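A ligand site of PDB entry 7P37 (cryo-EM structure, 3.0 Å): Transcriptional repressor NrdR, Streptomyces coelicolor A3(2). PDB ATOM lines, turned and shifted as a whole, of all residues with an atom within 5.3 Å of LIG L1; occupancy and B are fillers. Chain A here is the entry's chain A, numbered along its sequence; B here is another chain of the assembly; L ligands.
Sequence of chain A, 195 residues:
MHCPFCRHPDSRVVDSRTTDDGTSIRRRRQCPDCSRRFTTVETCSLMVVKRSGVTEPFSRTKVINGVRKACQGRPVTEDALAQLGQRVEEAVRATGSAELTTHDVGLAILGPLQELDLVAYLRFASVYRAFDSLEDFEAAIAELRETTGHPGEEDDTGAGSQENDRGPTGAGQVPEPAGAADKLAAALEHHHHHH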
ATOM      1  N   VAL A  48      11.863   5.220  19.390  1.00  0.00           N
ATOM      2  CA  VAL A  48      13.115   5.831  19.815  1.00  0.00           C
ATOM      3  C   VAL A  48      13.242   5.674  21.318  1.00  0.00           C
ATOM      4  O   VAL A  48      12.275   5.885  22.060  1.00  0.00           O
ATOM      5  CB  VAL A  48      13.205   7.321  19.394  1.00  0.00           C
ATOM      6  CG1 VAL A  48      13.377   7.430  17.895  1.00  0.00           C
ATOM      7  CG2 VAL A  48      11.973   8.082  19.853  1.00  0.00           C
ATOM      8  N   LYS A  50      14.529   6.948  24.666  1.00  0.00           N
ATOM      9  CA  LYS A  50      14.998   8.149  25.336  1.00  0.00           C
ATOM     10  C   LYS A  50      16.159   7.806  26.264  1.00  0.00           C
ATOM     11  O   LYS A  50      16.305   6.671  26.733  1.00  0.00           O
ATOM     12  CB  LYS A  50      13.863   8.792  26.127  1.00  0.00           C
ATOM     13  CG  LYS A  50      14.099  10.254  26.492  1.00  0.00           C
ATOM     14  CD  LYS A  50      12.925  10.826  27.265  1.00  0.00           C
ATOM     15  CE  LYS A  50      11.633  10.744  26.459  1.00  0.00           C
ATOM     16  NZ  LYS A  50      11.749  11.486  25.168  1.00  0.00           N
ATOM     17  N   ARG A  51      17.015   8.803  26.523  1.00  0.00           N
ATOM     18  CA  ARG A  51      18.144   8.598  27.424  1.00  0.00           C
ATOM     19  C   ARG A  51      17.705   8.272  28.848  1.00  0.00           C
ATOM     20  O   ARG A  51      18.518   7.765  29.626  1.00  0.00           O
ATOM     21  CB  ARG A  51      19.051   9.831  27.421  1.00  0.00           C
ATOM     22  CG  ARG A  51      19.902   9.964  26.171  1.00  0.00           C
ATOM     23  CD  ARG A  51      20.980  11.012  26.338  1.00  0.00           C
ATOM     24  NE  ARG A  51      20.424  12.346  26.557  1.00  0.00           N
ATOM     25  CZ  ARG A  51      21.143  13.463  26.589  1.00  0.00           C
ATOM     26  NH1 ARG A  51      22.453  13.441  26.423  1.00  0.00           N
ATOM     27  NH2 ARG A  51      20.523  14.617  26.804  1.00  0.00           N
ATOM     28  N   SER A  52      16.443   8.553  29.190  1.00  0.00           N
ATOM     29  CA  SER A  52      15.906   8.185  30.488  1.00  0.00           C
ATOM     30  C   SER A  52      15.484   6.727  30.571  1.00  0.00           C
ATOM     31  O   SER A  52      15.105   6.264  31.654  1.00  0.00           O
ATOM     32  CB  SER A  52      14.721   9.093  30.838  1.00  0.00           C
ATOM     33  OG  SER A  52      13.675   8.931  29.904  1.00  0.00           O
ATOM     34  N   GLU A  56       9.528   5.643  23.010  1.00  0.00           N
ATOM     35  CA  GLU A  56       8.342   6.340  22.534  1.00  0.00           C
ATOM     36  C   GLU A  56       8.307   6.334  21.025  1.00  0.00           C
ATOM     37  O   GLU A  56       9.350   6.238  20.368  1.00  0.00           O
ATOM     38  CB  GLU A  56       8.315   7.788  23.059  1.00  0.00           C
ATOM     39  CG  GLU A  56       9.576   8.577  22.815  1.00  0.00           C
ATOM     40  CD  GLU A  56       9.484   9.993  23.326  1.00  0.00           C
ATOM     41  OE1 GLU A  56       8.378  10.407  23.753  1.00  0.00           O
ATOM     42  OE2 GLU A  56      10.510  10.709  23.320  1.00  0.00           O
ATOM     43  N   PRO A  57       7.111   6.430  20.428  1.00  0.00           N
ATOM     44  CA  PRO A  57       7.012   6.375  18.954  1.00  0.00           C
ATOM     45  C   PRO A  57       7.783   7.513  18.294  1.00  0.00           C
ATOM     46  O   PRO A  57       7.848   8.630  18.812  1.00  0.00           O
ATOM     47  CB  PRO A  57       5.513   6.489  18.701  1.00  0.00           C
ATOM     48  CG  PRO A  57       4.929   7.042  19.963  1.00  0.00           C
ATOM     49  CD  PRO A  57       5.783   6.508  21.058  1.00  0.00           C
ATOM     50  N   PHE A  58       8.357   7.213  17.139  1.00  0.00           N
ATOM     51  CA  PHE A  58       9.109   8.210  16.384  1.00  0.00           C
ATOM     52  C   PHE A  58       8.190   9.331  15.925  1.00  0.00           C
ATOM     53  O   PHE A  58       7.059   9.085  15.481  1.00  0.00           O
ATOM     54  CB  PHE A  58       9.799   7.556  15.191  1.00  0.00           C
ATOM     55  CG  PHE A  58      10.703   8.478  14.425  1.00  0.00           C
ATOM     56  CD1 PHE A  58      10.227   9.232  13.366  1.00  0.00           C
ATOM     57  CD2 PHE A  58      12.040   8.591  14.756  1.00  0.00           C
ATOM     58  CE1 PHE A  58      11.052  10.076  12.663  1.00  0.00           C
ATOM     59  CE2 PHE A  58      12.886   9.429  14.054  1.00  0.00           C
ATOM     60  CZ  PHE A  58      12.389  10.177  13.005  1.00  0.00           C
ATOM     61  N   SER A  59       8.677  10.560  16.022  1.00  0.00           N
ATOM     62  CA  SER A  59       7.922  11.740  15.633  1.00  0.00           C
ATOM     63  C   SER A  59       8.799  12.648  14.782  1.00  0.00           C
ATOM     64  O   SER A  59       9.914  12.998  15.176  1.00  0.00           O
ATOM     65  CB  SER A  59       7.417  12.503  16.870  1.00  0.00           C
ATOM     66  OG  SER A  59       6.615  13.611  16.492  1.00  0.00           O
ATOM     67  N   LYS A  62       9.116  16.441  16.381  1.00  0.00           N
ATOM     68  CA  LYS A  62      10.180  16.700  17.344  1.00  0.00           C
ATOM     69  C   LYS A  62      11.520  16.928  16.656  1.00  0.00           C
ATOM     70  O   LYS A  62      12.297  17.805  17.074  1.00  0.00           O
ATOM     71  CB  LYS A  62      10.275  15.540  18.342  1.00  0.00           C
ATOM     72  CG  LYS A  62       9.023  15.354  19.172  1.00  0.00           C
ATOM     73  CD  LYS A  62       9.268  14.434  20.349  1.00  0.00           C
ATOM     74  CE  LYS A  62       8.010  14.260  21.175  1.00  0.00           C
ATOM     75  NZ  LYS A  62       8.229  13.379  22.357  1.00  0.00           N
ATOM     76  N   VAL A  63      11.809  16.167  15.593  1.00  0.00           N
ATOM     77  CA  VAL A  63      13.037  16.384  14.840  1.00  0.00           C
ATOM     78  C   VAL A  63      13.033  17.768  14.208  1.00  0.00           C
ATOM     79  O   VAL A  63      14.039  18.486  14.236  1.00  0.00           O
ATOM     80  CB  VAL A  63      13.204  15.282  13.772  1.00  0.00           C
ATOM     81  CG1 VAL A  63      14.334  15.613  12.827  1.00  0.00           C
ATOM     82  CG2 VAL A  63      13.431  13.933  14.442  1.00  0.00           C
ATOM     83  N   GLY A  66      13.644  20.372  16.924  1.00  0.00           N
ATOM     84  CA  GLY A  66      15.032  20.396  17.360  1.00  0.00           C
ATOM     85  C   GLY A  66      15.934  21.074  16.351  1.00  0.00           C
ATOM     86  O   GLY A  66      16.780  21.906  16.708  1.00  0.00           O
ATOM     87  N   THR A 102      18.226   7.700  20.466  1.00  0.00           N
ATOM     88  CA  THR A 102      18.206   9.089  20.022  1.00  0.00           C
ATOM     89  C   THR A 102      19.563   9.572  19.538  1.00  0.00           C
ATOM     90  O   THR A 102      19.627  10.514  18.752  1.00  0.00           O
ATOM     91  CB  THR A 102      17.707   9.988  21.150  1.00  0.00           C
ATOM     92  OG1 THR A 102      18.665   9.993  22.216  1.00  0.00           O
ATOM     93  CG2 THR A 102      16.359   9.497  21.674  1.00  0.00           C
ATOM     94  N   HIS A 103      20.645   8.948  20.006  1.00  0.00           N
ATOM     95  CA  HIS A 103      21.972   9.278  19.480  1.00  0.00           C
ATOM     96  C   HIS A 103      22.066   8.958  17.996  1.00  0.00           C
ATOM     97  O   HIS A 103      22.626   9.731  17.221  1.00  0.00           O
ATOM     98  CB  HIS A 103      23.045   8.535  20.275  1.00  0.00           C
ATOM     99  CG  HIS A 103      24.430   9.037  20.017  1.00  0.00           C
ATOM    100  ND1 HIS A 103      25.290   8.423  19.131  1.00  0.00           N
ATOM    101  CD2 HIS A 103      25.112  10.088  20.531  1.00  0.00           C
ATOM    102  CE1 HIS A 103      26.441   9.083  19.108  1.00  0.00           C
ATOM    103  NE2 HIS A 103      26.354  10.093  19.950  1.00  0.00           N
ATOM    104  N   VAL A 105      19.496   8.941  16.047  1.00  0.00           N
ATOM    105  CA  VAL A 105      18.653   9.954  15.418  1.00  0.00           C
ATOM    106  C   VAL A 105      19.450  11.217  15.150  1.00  0.00           C
ATOM    107  O   VAL A 105      19.381  11.811  14.074  1.00  0.00           O
ATOM    108  CB  VAL A 105      17.423  10.238  16.291  1.00  0.00           C
ATOM    109  CG1 VAL A 105      16.571  11.326  15.664  1.00  0.00           C
ATOM    110  CG2 VAL A 105      16.605   8.967  16.489  1.00  0.00           C
ATOM    111  N   ILE A 109      20.475  13.042  11.680  1.00  0.00           N
ATOM    112  CA  ILE A 109      20.223  14.465  11.434  1.00  0.00           C
ATOM    113  C   ILE A 109      21.486  15.145  10.941  1.00  0.00           C
ATOM    114  O   ILE A 109      21.431  16.073  10.120  1.00  0.00           O
ATOM    115  CB  ILE A 109      19.681  15.129  12.713  1.00  0.00           C
ATOM    116  CG1 ILE A 109      18.309  14.570  13.076  1.00  0.00           C
ATOM    117  CG2 ILE A 109      19.585  16.635  12.543  1.00  0.00           C
ATOM    118  CD1 ILE A 109      17.706  15.206  14.298  1.00  0.00           C
ATOM    119  N   PHE A 124      25.530  21.626  16.314  1.00  0.00           N
ATOM    120  CA  PHE A 124      24.818  20.380  16.573  1.00  0.00           C
ATOM    121  C   PHE A 124      25.778  19.200  16.711  1.00  0.00           C
ATOM    122  O   PHE A 124      25.605  18.334  17.580  1.00  0.00           O
ATOM    123  CB  PHE A 124      23.806  20.135  15.455  1.00  0.00           C
ATOM    124  CG  PHE A 124      22.759  19.107  15.770  1.00  0.00           C
ATOM    125  CD1 PHE A 124      21.686  19.434  16.593  1.00  0.00           C
ATOM    126  CD2 PHE A 124      22.814  17.841  15.227  1.00  0.00           C
ATOM    127  CE1 PHE A 124      20.708  18.505  16.874  1.00  0.00           C
ATOM    128  CE2 PHE A 124      21.836  16.913  15.508  1.00  0.00           C
ATOM    129  CZ  PHE A 124      20.785  17.234  16.333  1.00  0.00           C
ATOM    130  N   TYR A 128      26.613  16.159  19.331  1.00  0.00           N
ATOM    131  CA  TYR A 128      26.378  14.772  18.949  1.00  0.00           C
ATOM    132  C   TYR A 128      27.615  14.072  18.397  1.00  0.00           C
ATOM    133  O   TYR A 128      27.566  12.865  18.161  1.00  0.00           O
ATOM    134  CB  TYR A 128      25.229  14.690  17.950  1.00  0.00           C
ATOM    135  CG  TYR A 128      23.887  14.821  18.614  1.00  0.00           C
ATOM    136  CD1 TYR A 128      23.323  13.756  19.299  1.00  0.00           C
ATOM    137  CD2 TYR A 128      23.199  16.031  18.612  1.00  0.00           C
ATOM    138  CE1 TYR A 128      22.098  13.877  19.928  1.00  0.00           C
ATOM    139  CE2 TYR A 128      21.984  16.160  19.247  1.00  0.00           C
ATOM    140  CZ  TYR A 128      21.439  15.082  19.897  1.00  0.00           C
ATOM    141  OH  TYR A 128      20.221  15.213  20.518  1.00  0.00           O
ATOM    142  N   GLN B  72      25.934  19.899  28.393  1.00  0.00           N
ATOM    143  CA  GLN B  72      25.810  18.442  28.431  1.00  0.00           C
ATOM    144  C   GLN B  72      27.003  17.794  27.721  1.00  0.00           C
ATOM    145  O   GLN B  72      27.483  18.293  26.695  1.00  0.00           O
ATOM    146  CB  GLN B  72      24.493  17.991  27.785  1.00  0.00           C
ATOM    147  CG  GLN B  72      24.364  18.314  26.305  1.00  0.00           C
ATOM    148  CD  GLN B  72      23.057  17.831  25.724  1.00  0.00           C
ATOM    149  OE1 GLN B  72      22.386  16.969  26.287  1.00  0.00           O
ATOM    150  NE2 GLN B  72      22.671  18.400  24.589  1.00  0.00           N
HETATM  151  P1  LIG L   1      15.487  14.782  27.342  1.00  0.00           P
HETATM  152  O1  LIG L   1      15.338  13.548  28.154  1.00  0.00           O
HETATM  153  O2  LIG L   1      14.202  15.610  27.266  1.00  0.00           O
HETATM  154  O3  LIG L   1      16.634  15.690  27.815  1.00  0.00           O
HETATM  155  P2  LIG L   1      16.458  13.166  25.117  1.00  0.00           P
HETATM  156  O4  LIG L   1      17.215  12.323  26.046  1.00  0.00           O
HETATM  157  O5  LIG L   1      15.318  12.498  24.356  1.00  0.00           O
HETATM  158  O6  LIG L   1      15.839  14.442  25.826  1.00  0.00           O
HETATM  159  P3  LIG L   1      18.807  13.544  23.354  1.00  0.00           P
HETATM  160  O7  LIG L   1      19.286  12.185  23.649  1.00  0.00           O
HETATM  161  O8  LIG L   1      19.768  14.649  23.786  1.00  0.00           O
HETATM  162  O9  LIG L   1      17.392  13.834  24.012  1.00  0.00           O
HETATM  163  O10 LIG L   1      18.436  13.704  21.811  1.00  0.00           O
HETATM  164  C1  LIG L   1      17.136  14.183  21.432  1.00  0.00           C
HETATM  165  C2  LIG L   1      16.888  14.193  19.959  1.00  0.00           C
HETATM  166  O11 LIG L   1      16.164  12.997  19.626  1.00  0.00           O
HETATM  167  C3  LIG L   1      16.015  15.354  19.489  1.00  0.00           C
HETATM  168  O12 LIG L   1      16.832  16.451  19.069  1.00  0.00           O
HETATM  169  C4  LIG L   1      15.195  14.751  18.343  1.00  0.00           C
HETATM  170  O13 LIG L   1      15.808  14.894  17.068  1.00  0.00           O
HETATM  171  C5  LIG L   1      15.120  13.264  18.702  1.00  0.00           C
HETATM  172  N1  LIG L   1      13.864  12.842  19.299  1.00  0.00           N
HETATM  173  C6  LIG L   1      13.410  13.072  20.576  1.00  0.00           C
HETATM  174  N2  LIG L   1      12.228  12.574  20.826  1.00  0.00           N
HETATM  175  C7  LIG L   1      11.869  11.967  19.627  1.00  0.00           C
HETATM  176  C8  LIG L   1      10.718  11.261  19.222  1.00  0.00           C
HETATM  177  N3  LIG L   1       9.681  11.004  20.020  1.00  0.00           N
HETATM  178  N4  LIG L   1      10.691  10.806  17.954  1.00  0.00           N
HETATM  179  C9  LIG L   1      11.736  11.040  17.150  1.00  0.00           C
HETATM  180  N5  LIG L   1      12.863  11.684  17.417  1.00  0.00           N
HETATM  181  C10 LIG L   1      12.867  12.137  18.683  1.00  0.00           C
HETATM  182  P1  LG2 L   2      11.098  15.084  24.544  1.00  0.00           P
HETATM  183  O1  LG2 L   2      10.076  14.009  24.469  1.00  0.00           O
HETATM  184  O2  LG2 L   2      10.510  16.447  24.870  1.00  0.00           O
HETATM  185  O3  LG2 L   2      12.223  14.756  25.519  1.00  0.00           O
HETATM  186  P2  LG2 L   2      13.168  16.058  22.789  1.00  0.00           P
HETATM  187  O4  LG2 L   2      14.359  15.205  22.963  1.00  0.00           O
HETATM  188  O5  LG2 L   2      12.960  16.724  21.439  1.00  0.00           O
HETATM  189  O6  LG2 L   2      11.827  15.291  23.136  1.00  0.00           O
HETATM  190  P3  LG2 L   2      14.099  18.374  24.351  1.00  0.00           P
HETATM  191  O7  LG2 L   2      14.624  18.190  25.708  1.00  0.00           O
HETATM  192  O8  LG2 L   2      13.352  19.655  24.065  1.00  0.00           O
HETATM  193  O9  LG2 L   2      13.145  17.184  23.917  1.00  0.00           O
HETATM  194  O10 LG2 L   2      15.201  18.313  23.238  1.00  0.00           O
HETATM  195  C1  LG2 L   2      16.563  17.856  23.349  1.00  0.00           C
HETATM  196  C2  LG2 L   2      17.243  18.008  22.009  1.00  0.00           C
HETATM  197  O11 LG2 L   2      16.598  19.059  21.262  1.00  0.00           O
HETATM  198  C3  LG2 L   2      18.704  18.409  22.069  1.00  0.00           C
HETATM  199  O12 LG2 L   2      19.565  17.279  22.216  1.00  0.00           O
HETATM  200  C4  LG2 L   2      18.904  19.142  20.736  1.00  0.00           C
HETATM  201  O13 LG2 L   2      19.126  18.247  19.641  1.00  0.00           O
HETATM  202  C5  LG2 L   2      17.546  19.808  20.522  1.00  0.00           C
HETATM  203  N1  LG2 L   2      17.472  21.211  20.917  1.00  0.00           N
HETATM  204  C6  LG2 L   2      16.446  21.791  21.613  1.00  0.00           C
HETATM  205  N2  LG2 L   2      16.612  23.057  21.855  1.00  0.00           N
HETATM  206  C7  LG2 L   2      17.830  23.352  21.266  1.00  0.00           C
HETATM  207  C8  LG2 L   2      18.567  24.543  21.153  1.00  0.00           C
HETATM  208  N3  LG2 L   2      18.158  25.710  21.632  1.00  0.00           N
HETATM  209  N4  LG2 L   2      19.744  24.490  20.503  1.00  0.00           N
HETATM  210  C9  LG2 L   2      20.152  23.327  19.988  1.00  0.00           C
HETATM  211  N5  LG2 L   2      19.533  22.153  20.019  1.00  0.00           N
HETATM  212  C10 LG2 L   2      18.369  22.222  20.676  1.00  0.00           C
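OH of Tyr 128 sits at hydrogen-bond distance from O10 of LIG L1 (2.7 Å). An oxygen (O7) of LIG L1 sits at hydrogen-bond distance from the side-chain hydroxyl (OG1) of Thr 102 (2.7 Å). The backbone NH (N) of Ser 59 is in hydrogen-bond range of a nitrogen (N4) of LIG L1 (2.8 Å). The guanidinium group (NH2) of Arg 51 lies within salt-bridge range of an oxygen (O8) of LIG L1 (3.1 Å). O of Pro 57 sits at hydrogen-bond distance from N3 of LIG L1. The side-chain amino group of Lys 50 lies within salt-bridge range of an oxygen (O5) of LIG L1 (3.8 Å). The side-chain carboxylate of Glu 56 sits at hydrogen-bond distance from a nitrogen (N3) of LIG L1 (3.4 Å). The side-chain hydroxyl of Tyr 128 lies within hydrogen-bond range of an oxygen (O12) of LG2 L2, at 2.8 Å. The side-chain amino group of Lys 50 is in salt-bridge range of an oxygen (O1) of LG2 L2. The side-chain amino group (NZ) of Lys 62 lies within salt-bridge range of an oxygen (O1) of LG2 L2 (2.9 Å).
An oxygen (O12) of LIG L1 is in hydrogen-bond range of an oxygen (O13) of LG2 L2, 3.0 Å away.
The side-chain amide oxygen of Gln 72 of chain B sits at hydrogen-bond distance from the guanidinium group of Arg 51, 3.0 Å away. The side-chain carboxylate (OE1) of Glu 56 is in salt-bridge range of the side-chain amino group (NZ) of Lys 50. The side-chain carboxylate of Glu 56 is in salt-bridge range of the side-chain amino group of Lys 62, 3.3 Å away. The backbone carbonyl oxygen (O) of Glu 56 lies within hydrogen-bond range of the backbone NH (N) of Val 48, at 2.9 Å.
Val 48 touches LIG L1 (CG2 to C8, 3.5 Å). Phe 58 touches LIG L1 (CA to N4, 3.4 Å). Lys 62 touches LIG L1. Val 63 touches LIG L1. CG1 of Val 105 touches C5 of LIG L1 (3.9 Å). CD1 of Ile 109 touches O13 of LIG L1 (3.4 Å). Hydrophobic or aromatic side chains within 4 Å of LIG L1: Val 48, Phe 58, Val 63, Val 105, Ile 109 and Tyr 128. Of the 18 residues printed, 13 come within 4 Å of LIG L1. The nearest printed residue that does not touch LIG L1 is Gln 72 of chain B (4.3 Å).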
